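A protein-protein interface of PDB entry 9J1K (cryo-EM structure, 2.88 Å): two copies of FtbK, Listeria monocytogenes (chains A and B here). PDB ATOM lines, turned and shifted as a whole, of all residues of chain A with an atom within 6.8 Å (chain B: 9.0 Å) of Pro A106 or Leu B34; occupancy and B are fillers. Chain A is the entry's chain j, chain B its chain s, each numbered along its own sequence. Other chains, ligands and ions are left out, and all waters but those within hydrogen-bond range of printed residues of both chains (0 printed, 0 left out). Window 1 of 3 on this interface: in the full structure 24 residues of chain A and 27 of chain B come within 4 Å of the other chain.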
ATOM      1  N   PHE A  83      -9.378 -10.031 -17.151  1.00  0.00           N
ATOM      2  CA  PHE A  83      -8.130  -9.604 -17.774  1.00  0.00           C
ATOM      3  C   PHE A  83      -7.902  -8.106 -17.611  1.00  0.00           C
ATOM      4  O   PHE A  83      -6.781  -7.673 -17.318  1.00  0.00           O
ATOM      5  CB  PHE A  83      -8.140  -9.988 -19.253  1.00  0.00           C
ATOM      6  CG  PHE A  83      -6.964  -9.470 -20.027  1.00  0.00           C
ATOM      7  CD1 PHE A  83      -5.694  -9.971 -19.804  1.00  0.00           C
ATOM      8  CD2 PHE A  83      -7.132  -8.489 -20.988  1.00  0.00           C
ATOM      9  CE1 PHE A  83      -4.613  -9.497 -20.520  1.00  0.00           C
ATOM     10  CE2 PHE A  83      -6.056  -8.011 -21.706  1.00  0.00           C
ATOM     11  CZ  PHE A  83      -4.795  -8.516 -21.473  1.00  0.00           C
ATOM     12  N   LEU A  84      -8.949  -7.301 -17.795  1.00  0.00           N
ATOM     13  CA  LEU A  84      -8.768  -5.852 -17.824  1.00  0.00           C
ATOM     14  C   LEU A  84      -8.474  -5.290 -16.438  1.00  0.00           C
ATOM     15  O   LEU A  84      -7.579  -4.452 -16.281  1.00  0.00           O
ATOM     16  CB  LEU A  84     -10.006  -5.183 -18.417  1.00  0.00           C
ATOM     17  CG  LEU A  84     -10.091  -5.163 -19.941  1.00  0.00           C
ATOM     18  CD1 LEU A  84     -11.346  -4.441 -20.394  1.00  0.00           C
ATOM     19  CD2 LEU A  84      -8.853  -4.514 -20.532  1.00  0.00           C
ATOM     20  N   PHE A  85      -9.213  -5.732 -15.425  1.00  0.00           N
ATOM     21  CA  PHE A  85      -9.149  -5.129 -14.098  1.00  0.00           C
ATOM     22  C   PHE A  85      -8.138  -5.886 -13.244  1.00  0.00           C
ATOM     23  O   PHE A  85      -8.378  -7.032 -12.853  1.00  0.00           O
ATOM     24  CB  PHE A  85     -10.529  -5.124 -13.450  1.00  0.00           C
ATOM     25  CG  PHE A  85     -11.488  -4.165 -14.090  1.00  0.00           C
ATOM     26  CD1 PHE A  85     -12.292  -4.568 -15.140  1.00  0.00           C
ATOM     27  CD2 PHE A  85     -11.576  -2.856 -13.649  1.00  0.00           C
ATOM     28  CE1 PHE A  85     -13.172  -3.686 -15.735  1.00  0.00           C
ATOM     29  CE2 PHE A  85     -12.453  -1.970 -14.240  1.00  0.00           C
ATOM     30  CZ  PHE A  85     -13.252  -2.386 -15.284  1.00  0.00           C
ATOM     31  N   GLN A  86      -7.013  -5.243 -12.955  1.00  0.00           N
ATOM     32  CA  GLN A  86      -5.970  -5.795 -12.106  1.00  0.00           C
ATOM     33  C   GLN A  86      -5.779  -4.908 -10.884  1.00  0.00           C
ATOM     34  O   GLN A  86      -6.308  -3.797 -10.800  1.00  0.00           O
ATOM     35  CB  GLN A  86      -4.651  -5.942 -12.874  1.00  0.00           C
ATOM     36  CG  GLN A  86      -4.815  -6.496 -14.275  1.00  0.00           C
ATOM     37  CD  GLN A  86      -4.491  -7.973 -14.355  1.00  0.00           C
ATOM     38  OE1 GLN A  86      -3.722  -8.495 -13.549  1.00  0.00           O
ATOM     39  NE2 GLN A  86      -5.080  -8.656 -15.328  1.00  0.00           N
ATOM     40  N   ARG A  87      -5.010  -5.421  -9.922  1.00  0.00           N
ATOM     41  CA  ARG A  87      -4.786  -4.688  -8.680  1.00  0.00           C
ATOM     42  C   ARG A  87      -4.026  -3.390  -8.924  1.00  0.00           C
ATOM     43  O   ARG A  87      -4.371  -2.346  -8.359  1.00  0.00           O
ATOM     44  CB  ARG A  87      -4.029  -5.563  -7.684  1.00  0.00           C
ATOM     45  CG  ARG A  87      -4.887  -6.601  -6.995  1.00  0.00           C
ATOM     46  CD  ARG A  87      -5.394  -6.081  -5.666  1.00  0.00           C
ATOM     47  NE  ARG A  87      -6.553  -6.833  -5.205  1.00  0.00           N
ATOM     48  CZ  ARG A  87      -7.529  -6.327  -4.465  1.00  0.00           C
ATOM     49  NH1 ARG A  87      -7.522  -5.060  -4.087  1.00  0.00           N
ATOM     50  NH2 ARG A  87      -8.536  -7.111  -4.098  1.00  0.00           N
ATOM     51  N   ASP A  88      -2.993  -3.434  -9.759  1.00  0.00           N
ATOM     52  CA  ASP A  88      -2.102  -2.304  -9.960  1.00  0.00           C
ATOM     53  C   ASP A  88      -2.176  -1.816 -11.400  1.00  0.00           C
ATOM     54  O   ASP A  88      -2.660  -2.513 -12.294  1.00  0.00           O
ATOM     55  CB  ASP A  88      -0.657  -2.676  -9.608  1.00  0.00           C
ATOM     56  CG  ASP A  88      -0.300  -4.082 -10.034  1.00  0.00           C
ATOM     57  OD1 ASP A  88      -1.173  -4.768 -10.606  1.00  0.00           O
ATOM     58  OD2 ASP A  88       0.851  -4.504  -9.797  1.00  0.00           O
ATOM     59  N   SER A  89      -1.686  -0.596 -11.606  1.00  0.00           N
ATOM     60  CA  SER A  89      -1.696   0.009 -12.929  1.00  0.00           C
ATOM     61  C   SER A  89      -0.775  -0.752 -13.874  1.00  0.00           C
ATOM     62  O   SER A  89       0.199  -1.380 -13.454  1.00  0.00           O
ATOM     63  CB  SER A  89      -1.263   1.472 -12.844  1.00  0.00           C
ATOM     64  OG  SER A  89       0.098   1.575 -12.468  1.00  0.00           O
ATOM     65  N   TYR A  90      -1.091  -0.693 -15.167  1.00  0.00           N
ATOM     66  CA  TYR A  90      -0.257  -1.378 -16.150  1.00  0.00           C
ATOM     67  C   TYR A  90       0.004  -0.464 -17.337  1.00  0.00           C
ATOM     68  O   TYR A  90      -0.278   0.735 -17.261  1.00  0.00           O
ATOM     69  CB  TYR A  90      -0.903  -2.688 -16.598  1.00  0.00           C
ATOM     70  CG  TYR A  90      -2.379  -2.594 -16.889  1.00  0.00           C
ATOM     71  CD1 TYR A  90      -2.839  -2.094 -18.097  1.00  0.00           C
ATOM     72  CD2 TYR A  90      -3.316  -3.018 -15.957  1.00  0.00           C
ATOM     73  CE1 TYR A  90      -4.187  -2.012 -18.367  1.00  0.00           C
ATOM     74  CE2 TYR A  90      -4.666  -2.939 -16.219  1.00  0.00           C
ATOM     75  CZ  TYR A  90      -5.096  -2.436 -17.425  1.00  0.00           C
ATOM     76  OH  TYR A  90      -6.442  -2.356 -17.691  1.00  0.00           O
ATOM     77  N   VAL A 104      -1.654   3.269 -17.095  1.00  0.00           N
ATOM     78  CA  VAL A 104      -3.074   3.512 -16.889  1.00  0.00           C
ATOM     79  C   VAL A 104      -3.644   2.572 -15.838  1.00  0.00           C
ATOM     80  O   VAL A 104      -3.067   1.531 -15.502  1.00  0.00           O
ATOM     81  CB  VAL A 104      -3.879   3.368 -18.198  1.00  0.00           C
ATOM     82  CG1 VAL A 104      -3.316   4.267 -19.283  1.00  0.00           C
ATOM     83  CG2 VAL A 104      -3.884   1.921 -18.652  1.00  0.00           C
ATOM     84  N   HIS A 105      -4.805   2.977 -15.320  1.00  0.00           N
ATOM     85  CA  HIS A 105      -5.692   2.181 -14.491  1.00  0.00           C
ATOM     86  C   HIS A 105      -7.040   2.055 -15.189  1.00  0.00           C
ATOM     87  O   HIS A 105      -7.542   3.050 -15.728  1.00  0.00           O
ATOM     88  CB  HIS A 105      -5.886   2.826 -13.109  1.00  0.00           C
ATOM     89  CG  HIS A 105      -5.060   2.211 -12.025  1.00  0.00           C
ATOM     90  ND1 HIS A 105      -4.352   2.962 -11.113  1.00  0.00           N
ATOM     91  CD2 HIS A 105      -4.848   0.916 -11.692  1.00  0.00           C
ATOM     92  CE1 HIS A 105      -3.728   2.156 -10.272  1.00  0.00           C
ATOM     93  NE2 HIS A 105      -4.014   0.910 -10.601  1.00  0.00           N
ATOM     94  N   PRO A 106      -7.660   0.881 -15.196  1.00  0.00           N
ATOM     95  CA  PRO A 106      -8.947   0.739 -15.883  1.00  0.00           C
ATOM     96  C   PRO A 106     -10.066   1.448 -15.136  1.00  0.00           C
ATOM     97  O   PRO A 106      -9.975   1.740 -13.942  1.00  0.00           O
ATOM     98  CB  PRO A 106      -9.179  -0.776 -15.923  1.00  0.00           C
ATOM     99  CG  PRO A 106      -8.085  -1.399 -15.105  1.00  0.00           C
ATOM    100  CD  PRO A 106      -7.282  -0.327 -14.451  1.00  0.00           C
ATOM    101  N   LYS A 107     -11.140   1.730 -15.872  1.00  0.00           N
ATOM    102  CA  LYS A 107     -12.330   2.362 -15.330  1.00  0.00           C
ATOM    103  C   LYS A 107     -13.543   1.464 -15.545  1.00  0.00           C
ATOM    104  O   LYS A 107     -13.574   0.675 -16.494  1.00  0.00           O
ATOM    105  CB  LYS A 107     -12.587   3.726 -15.983  1.00  0.00           C
ATOM    106  CG  LYS A 107     -11.424   4.695 -15.879  1.00  0.00           C
ATOM    107  CD  LYS A 107     -11.819   6.077 -16.370  1.00  0.00           C
ATOM    108  CE  LYS A 107     -13.039   6.598 -15.632  1.00  0.00           C
ATOM    109  NZ  LYS A 107     -13.088   8.085 -15.625  1.00  0.00           N
ATOM    110  N   PRO A 108     -14.552   1.554 -14.679  1.00  0.00           N
ATOM    111  CA  PRO A 108     -15.731   0.686 -14.823  1.00  0.00           C
ATOM    112  C   PRO A 108     -16.483   0.980 -16.110  1.00  0.00           C
ATOM    113  O   PRO A 108     -16.924   2.106 -16.351  1.00  0.00           O
ATOM    114  CB  PRO A 108     -16.570   1.024 -13.586  1.00  0.00           C
ATOM    115  CG  PRO A 108     -15.604   1.618 -12.617  1.00  0.00           C
ATOM    116  CD  PRO A 108     -14.612   2.361 -13.449  1.00  0.00           C
ATOM    117  N   ILE A 123     -14.018   0.773 -23.643  1.00  0.00           N
ATOM    118  CA  ILE A 123     -13.114   0.721 -22.503  1.00  0.00           C
ATOM    119  C   ILE A 123     -12.473   2.085 -22.303  1.00  0.00           C
ATOM    120  O   ILE A 123     -12.090   2.761 -23.267  1.00  0.00           O
ATOM    121  CB  ILE A 123     -12.048  -0.367 -22.704  1.00  0.00           C
ATOM    122  CG1 ILE A 123     -12.631  -1.550 -23.472  1.00  0.00           C
ATOM    123  CG2 ILE A 123     -11.503  -0.823 -21.364  1.00  0.00           C
ATOM    124  CD1 ILE A 123     -11.597  -2.564 -23.901  1.00  0.00           C
ATOM    125  N   GLU A 124     -12.364   2.506 -21.048  1.00  0.00           N
ATOM    126  CA  GLU A 124     -11.746   3.777 -20.709  1.00  0.00           C
ATOM    127  C   GLU A 124     -10.648   3.534 -19.687  1.00  0.00           C
ATOM    128  O   GLU A 124     -10.899   2.941 -18.633  1.00  0.00           O
ATOM    129  CB  GLU A 124     -12.779   4.766 -20.161  1.00  0.00           C
ATOM    130  CG  GLU A 124     -13.370   5.682 -21.218  1.00  0.00           C
ATOM    131  CD  GLU A 124     -14.798   6.083 -20.912  1.00  0.00           C
ATOM    132  OE1 GLU A 124     -15.093   6.385 -19.737  1.00  0.00           O
ATOM    133  OE2 GLU A 124     -15.626   6.096 -21.846  1.00  0.00           O
ATOM    134  N   PHE A 125      -9.439   3.984 -20.001  1.00  0.00           N
ATOM    135  CA  PHE A 125      -8.293   3.863 -19.113  1.00  0.00           C
ATOM    136  C   PHE A 125      -7.920   5.252 -18.622  1.00  0.00           C
ATOM    137  O   PHE A 125      -7.646   6.146 -19.427  1.00  0.00           O
ATOM    138  CB  PHE A 125      -7.106   3.216 -19.827  1.00  0.00           C
ATOM    139  CG  PHE A 125      -7.413   1.879 -20.432  1.00  0.00           C
ATOM    140  CD1 PHE A 125      -7.947   1.785 -21.704  1.00  0.00           C
ATOM    141  CD2 PHE A 125      -7.154   0.715 -19.732  1.00  0.00           C
ATOM    142  CE1 PHE A 125      -8.225   0.555 -22.262  1.00  0.00           C
ATOM    143  CE2 PHE A 125      -7.430  -0.517 -20.285  1.00  0.00           C
ATOM    144  CZ  PHE A 125      -7.966  -0.596 -21.552  1.00  0.00           C
ATOM    145  N   ASP A 126      -7.916   5.431 -17.306  1.00  0.00           N
ATOM    146  CA  ASP A 126      -7.466   6.681 -16.719  1.00  0.00           C
ATOM    147  C   ASP A 126      -5.947   6.660 -16.622  1.00  0.00           C
ATOM    148  O   ASP A 126      -5.375   5.792 -15.951  1.00  0.00           O
ATOM    149  CB  ASP A 126      -8.096   6.880 -15.342  1.00  0.00           C
ATOM    150  CG  ASP A 126      -7.897   8.282 -14.808  1.00  0.00           C
ATOM    151  OD1 ASP A 126      -8.192   9.247 -15.544  1.00  0.00           O
ATOM    152  OD2 ASP A 126      -7.447   8.420 -13.652  1.00  0.00           O
ATOM    153  N   GLN B  30     -22.701  -6.229 -13.708  1.00  0.00           N
ATOM    154  CA  GLN B  30     -21.962  -4.984 -13.819  1.00  0.00           C
ATOM    155  C   GLN B  30     -20.461  -5.254 -13.845  1.00  0.00           C
ATOM    156  O   GLN B  30     -19.980  -6.300 -13.401  1.00  0.00           O
ATOM    157  CB  GLN B  30     -22.302  -4.052 -12.656  1.00  0.00           C
ATOM    158  CG  GLN B  30     -22.502  -2.603 -13.055  1.00  0.00           C
ATOM    159  CD  GLN B  30     -22.597  -1.685 -11.855  1.00  0.00           C
ATOM    160  OE1 GLN B  30     -22.464  -2.123 -10.713  1.00  0.00           O
ATOM    161  NE2 GLN B  30     -22.826  -0.402 -12.108  1.00  0.00           N
ATOM    162  N   SER B  31     -19.718  -4.290 -14.378  1.00  0.00           N
ATOM    163  CA  SER B  31     -18.272  -4.382 -14.384  1.00  0.00           C
ATOM    164  C   SER B  31     -17.731  -4.206 -12.969  1.00  0.00           C
ATOM    165  O   SER B  31     -18.393  -3.619 -12.111  1.00  0.00           O
ATOM    166  CB  SER B  31     -17.676  -3.322 -15.304  1.00  0.00           C
ATOM    167  OG  SER B  31     -17.434  -2.120 -14.598  1.00  0.00           O
ATOM    168  N   PRO B  32     -16.534  -4.725 -12.694  1.00  0.00           N
ATOM    169  CA  PRO B  32     -15.917  -4.478 -11.388  1.00  0.00           C
ATOM    170  C   PRO B  32     -15.744  -2.987 -11.145  1.00  0.00           C
ATOM    171  O   PRO B  32     -15.346  -2.235 -12.036  1.00  0.00           O
ATOM    172  CB  PRO B  32     -14.567  -5.196 -11.491  1.00  0.00           C
ATOM    173  CG  PRO B  32     -14.781  -6.242 -12.527  1.00  0.00           C
ATOM    174  CD  PRO B  32     -15.734  -5.647 -13.517  1.00  0.00           C
ATOM    175  N   GLN B  33     -16.048  -2.564  -9.922  1.00  0.00           N
ATOM    176  CA  GLN B  33     -16.030  -1.150  -9.553  1.00  0.00           C
ATOM    177  C   GLN B  33     -14.674  -0.846  -8.926  1.00  0.00           C
ATOM    178  O   GLN B  33     -14.487  -0.967  -7.716  1.00  0.00           O
ATOM    179  CB  GLN B  33     -17.176  -0.823  -8.606  1.00  0.00           C
ATOM    180  CG  GLN B  33     -18.533  -1.268  -9.112  1.00  0.00           C
ATOM    181  CD  GLN B  33     -18.991  -0.468 -10.312  1.00  0.00           C
ATOM    182  OE1 GLN B  33     -19.109   0.755 -10.249  1.00  0.00           O
ATOM    183  NE2 GLN B  33     -19.250  -1.155 -11.417  1.00  0.00           N
ATOM    184  N   LEU B  34     -13.722  -0.445  -9.762  1.00  0.00           N
ATOM    185  CA  LEU B  34     -12.389  -0.115  -9.278  1.00  0.00           C
ATOM    186  C   LEU B  34     -12.406   1.251  -8.604  1.00  0.00           C
ATOM    187  O   LEU B  34     -12.602   2.276  -9.266  1.00  0.00           O
ATOM    188  CB  LEU B  34     -11.390  -0.134 -10.431  1.00  0.00           C
ATOM    189  CG  LEU B  34      -9.916  -0.154 -10.030  1.00  0.00           C
ATOM    190  CD1 LEU B  34      -9.625  -1.346  -9.137  1.00  0.00           C
ATOM    191  CD2 LEU B  34      -9.031  -0.178 -11.262  1.00  0.00           C
ATOM    192  N   SER B  35     -12.199   1.266  -7.292  1.00  0.00           N
ATOM    193  CA  SER B  35     -12.130   2.492  -6.515  1.00  0.00           C
ATOM    194  C   SER B  35     -10.677   2.794  -6.181  1.00  0.00           C
ATOM    195  O   SER B  35      -9.903   1.889  -5.846  1.00  0.00           O
ATOM    196  CB  SER B  35     -12.948   2.383  -5.228  1.00  0.00           C
ATOM    197  OG  SER B  35     -13.195   3.662  -4.674  1.00  0.00           O
ATOM    198  N   MET B  36     -10.318   4.070  -6.268  1.00  0.00           N
ATOM    199  CA  MET B  36      -8.934   4.495  -6.151  1.00  0.00           C
ATOM    200  C   MET B  36      -8.891   5.853  -5.471  1.00  0.00           C
ATOM    201  O   MET B  36      -9.745   6.707  -5.725  1.00  0.00           O
ATOM    202  CB  MET B  36      -8.276   4.561  -7.532  1.00  0.00           C
ATOM    203  CG  MET B  36      -6.824   4.140  -7.572  1.00  0.00           C
ATOM    204  SD  MET B  36      -6.062   4.528  -9.159  1.00  0.00           S
ATOM    205  CE  MET B  36      -7.502   4.660 -10.219  1.00  0.00           C
ATOM    206  N   GLU B  37      -7.898   6.046  -4.610  1.00  0.00           N
ATOM    207  CA  GLU B  37      -7.697   7.308  -3.912  1.00  0.00           C
ATOM    208  C   GLU B  37      -6.508   8.032  -4.525  1.00  0.00           C
ATOM    209  O   GLU B  37      -5.421   7.458  -4.645  1.00  0.00           O
ATOM    210  CB  GLU B  37      -7.472   7.082  -2.417  1.00  0.00           C
ATOM    211  CG  GLU B  37      -8.752   6.868  -1.629  1.00  0.00           C
ATOM    212  CD  GLU B  37      -9.267   8.149  -1.003  1.00  0.00           C
ATOM    213  OE1 GLU B  37      -8.488   9.119  -0.906  1.00  0.00           O
ATOM    214  OE2 GLU B  37     -10.451   8.185  -0.608  1.00  0.00           O
ATOM    215  N   GLY B  50      -3.517   5.714  -4.555  1.00  0.00           N
ATOM    216  CA  GLY B  50      -3.396   4.806  -3.436  1.00  0.00           C
ATOM    217  C   GLY B  50      -3.671   3.375  -3.856  1.00  0.00           C
ATOM    218  O   GLY B  50      -3.780   3.046  -5.038  1.00  0.00           O
ATOM    219  N   MET B  51      -3.777   2.503  -2.856  1.00  0.00           N
ATOM    220  CA  MET B  51      -4.078   1.107  -3.136  1.00  0.00           C
ATOM    221  C   MET B  51      -5.500   0.981  -3.664  1.00  0.00           C
ATOM    222  O   MET B  51      -6.446   1.498  -3.062  1.00  0.00           O
ATOM    223  CB  MET B  51      -3.902   0.247  -1.887  1.00  0.00           C
ATOM    224  CG  MET B  51      -4.120  -1.236  -2.154  1.00  0.00           C
ATOM    225  SD  MET B  51      -3.940  -2.320  -0.722  1.00  0.00           S
ATOM    226  CE  MET B  51      -4.061  -1.152   0.626  1.00  0.00           C
ATOM    227  N   THR B  52      -5.648   0.296  -4.791  1.00  0.00           N
ATOM    228  CA  THR B  52      -6.951   0.135  -5.414  1.00  0.00           C
ATOM    229  C   THR B  52      -7.794  -0.869  -4.640  1.00  0.00           C
ATOM    230  O   THR B  52      -7.276  -1.775  -3.982  1.00  0.00           O
ATOM    231  CB  THR B  52      -6.801  -0.326  -6.862  1.00  0.00           C
ATOM    232  OG1 THR B  52      -6.258  -1.651  -6.887  1.00  0.00           O
ATOM    233  CG2 THR B  52      -5.871   0.605  -7.620  1.00  0.00           C
ATOM    234  N   GLN B  53      -9.111  -0.698  -4.723  1.00  0.00           N
ATOM    235  CA  GLN B  53     -10.056  -1.628  -4.125  1.00  0.00           C
ATOM    236  C   GLN B  53     -11.193  -1.878  -5.103  1.00  0.00           C
ATOM    237  O   GLN B  53     -11.312  -1.211  -6.133  1.00  0.00           O
ATOM    238  CB  GLN B  53     -10.600  -1.100  -2.792  1.00  0.00           C
ATOM    239  CG  GLN B  53     -10.941   0.375  -2.795  1.00  0.00           C
ATOM    240  CD  GLN B  53     -11.656   0.803  -1.530  1.00  0.00           C
ATOM    241  OE1 GLN B  53     -12.529   0.096  -1.029  1.00  0.00           O
ATOM    242  NE2 GLN B  53     -11.286   1.965  -1.007  1.00  0.00           N
ATOM    243  N   PHE B  54     -12.037  -2.852  -4.776  1.00  0.00           N
ATOM    244  CA  PHE B  54     -13.172  -3.214  -5.618  1.00  0.00           C
ATOM    245  C   PHE B  54     -14.451  -3.074  -4.803  1.00  0.00           C
ATOM    246  O   PHE B  54     -14.677  -3.830  -3.853  1.00  0.00           O
ATOM    247  CB  PHE B  54     -13.012  -4.628  -6.172  1.00  0.00           C
ATOM    248  CG  PHE B  54     -11.907  -4.755  -7.179  1.00  0.00           C
ATOM    249  CD1 PHE B  54     -10.623  -5.087  -6.783  1.00  0.00           C
ATOM    250  CD2 PHE B  54     -12.148  -4.527  -8.523  1.00  0.00           C
ATOM    251  CE1 PHE B  54      -9.605  -5.198  -7.708  1.00  0.00           C
ATOM    252  CE2 PHE B  54     -11.133  -4.637  -9.451  1.00  0.00           C
ATOM    253  CZ  PHE B  54      -9.861  -4.973  -9.044  1.00  0.00           C
ATOM    254  N   LYS B  55     -15.279  -2.106  -5.182  1.00  0.00           N
ATOM    255  CA  LYS B  55     -16.532  -1.852  -4.499  1.00  0.00           C
ATOM    256  C   LYS B  55     -17.562  -2.922  -4.854  1.00  0.00           C
ATOM    257  O   LYS B  55     -17.404  -3.645  -5.841  1.00  0.00           O
ATOM    258  CB  LYS B  55     -17.056  -0.466  -4.870  1.00  0.00           C
ATOM    259  CG  LYS B  55     -16.028   0.637  -4.727  1.00  0.00           C
ATOM    260  CD  LYS B  55     -16.052   1.235  -3.332  1.00  0.00           C
ATOM    261  CE  LYS B  55     -17.033   2.391  -3.246  1.00  0.00           C
ATOM    262  NZ  LYS B  55     -17.041   3.201  -4.494  1.00  0.00           N
ATOM    263  N   PRO B  56     -18.619  -3.054  -4.051  1.00  0.00           N
ATOM    264  CA  PRO B  56     -19.700  -3.979  -4.406  1.00  0.00           C
ATOM    265  C   PRO B  56     -20.305  -3.625  -5.754  1.00  0.00           C
ATOM    266  O   PRO B  56     -20.417  -2.452  -6.117  1.00  0.00           O
ATOM    267  CB  PRO B  56     -20.716  -3.786  -3.275  1.00  0.00           C
ATOM    268  CG  PRO B  56     -19.923  -3.271  -2.137  1.00  0.00           C
ATOM    269  CD  PRO B  56     -18.833  -2.437  -2.730  1.00  0.00           C
ATOM    270  N   PHE B  57     -20.697  -4.650  -6.503  1.00  0.00           N
ATOM    271  CA  PHE B  57     -21.262  -4.411  -7.827  1.00  0.00           C
ATOM    272  C   PHE B  57     -22.666  -5.010  -7.907  1.00  0.00           C
ATOM    273  O   PHE B  57     -23.219  -5.483  -6.913  1.00  0.00           O
ATOM    274  CB  PHE B  57     -20.328  -4.933  -8.925  1.00  0.00           C
ATOM    275  CG  PHE B  57     -20.156  -6.422  -8.936  1.00  0.00           C
ATOM    276  CD1 PHE B  57     -19.166  -7.023  -8.181  1.00  0.00           C
ATOM    277  CD2 PHE B  57     -20.957  -7.219  -9.734  1.00  0.00           C
ATOM    278  CE1 PHE B  57     -18.995  -8.392  -8.200  1.00  0.00           C
ATOM    279  CE2 PHE B  57     -20.791  -8.589  -9.757  1.00  0.00           C
ATOM    280  CZ  PHE B  57     -19.809  -9.175  -8.989  1.00  0.00           C
ATOM    281  N   GLY B 130     -17.566  -7.815  -3.551  1.00  0.00           N
ATOM    282  CA  GLY B 130     -16.750  -7.300  -4.626  1.00  0.00           C
ATOM    283  C   GLY B 130     -16.205  -8.339  -5.578  1.00  0.00           C
ATOM    284  O   GLY B 130     -15.426  -7.983  -6.472  1.00  0.00           O
ATOM    285  N   ARG B 272     -13.087 -12.143 -10.417  1.00  0.00           N
ATOM    286  CA  ARG B 272     -13.378 -10.721 -10.536  1.00  0.00           C
ATOM    287  C   ARG B 272     -14.569 -10.483 -11.457  1.00  0.00           C
ATOM    288  O   ARG B 272     -14.827 -11.269 -12.368  1.00  0.00           O
ATOM    289  CB  ARG B 272     -12.153  -9.967 -11.053  1.00  0.00           C
ATOM    290  CG  ARG B 272     -12.267  -8.461 -10.941  1.00  0.00           C
ATOM    291  CD  ARG B 272     -12.174  -8.017  -9.494  1.00  0.00           C
ATOM    292  NE  ARG B 272     -10.951  -8.489  -8.858  1.00  0.00           N
ATOM    293  CZ  ARG B 272     -10.787  -8.607  -7.548  1.00  0.00           C
ATOM    294  NH1 ARG B 272     -11.756  -8.302  -6.700  1.00  0.00           N
ATOM    295  NH2 ARG B 272      -9.622  -9.040  -7.075  1.00  0.00           N
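The backbone carbonyl oxygen of Arg A87 lies within hydrogen-bond range of the side-chain hydroxyl of Thr B52, 2.5 Å away. ND1 of His A105 sits at hydrogen-bond distance from SD of Met B36 (3.0 Å).
NE2 of His A105 lies within hydrogen-bond range of N of Ser A89, 2.9 Å away. O of His A105 lies within hydrogen-bond range of N of Asp A126 (2.9 Å). The backbone carbonyl oxygen (O) of Ser B31 is in hydrogen-bond range of the side-chain amide nitrogen (NE2) of Gln B33.
Among the printed residues, merely in contact across the chains: Pro A108 with Ser B31 (3.3 Å), Pro A106 with Leu B34 (3.4 Å), His A105 with Thr B52 (3.5 Å), Phe A85 with Pro B32 (3.6 Å), Arg A87 with Arg B272 (3.7 Å), Pro A108 with Pro B32 (3.8 Å), Arg A87 with Phe B54 (3.96 Å) and Pro A108 with Leu B34 (3.99 Å).
Of the printed residues of chain B, Arg A87 touches Thr B52, Phe B54 and Arg B272. Pro A106 touches just one residue of chain B: Leu B34 (3.4 Å). Of the printed residues of chain B, Pro A108 touches Ser B31 (3.3 Å), Pro B32 (3.8 Å) and Leu B34 (3.99 Å). Printed residues of chain A within 4 Å of Leu B34: Pro A106 and Pro A108. The nearest residue of chain B that does not touch Pro A106 is Met B36 (5.3 Å).
Printed residues of chain B that touch a printed residue of chain A: Ser B31, Pro B32, Leu B34, Met B36, Thr B52, Phe B54 and Arg B272. Hydrophobic or aromatic side chains of chain B within 4 Å of the printed part of chain A: Pro B32, Leu B34, Met B36 and Phe B54. Among the printed residues, 10 pairs touch across the chains. Among the printed residues, no Asp or Glu carboxylate lies within 4 Å of a Lys or Arg side-chain nitrogen of the other chain.
No position is printed for both chains. Of the 10 pairs that touch across the chains among the printed residues, none has its exchanged pair printed and touching as well.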
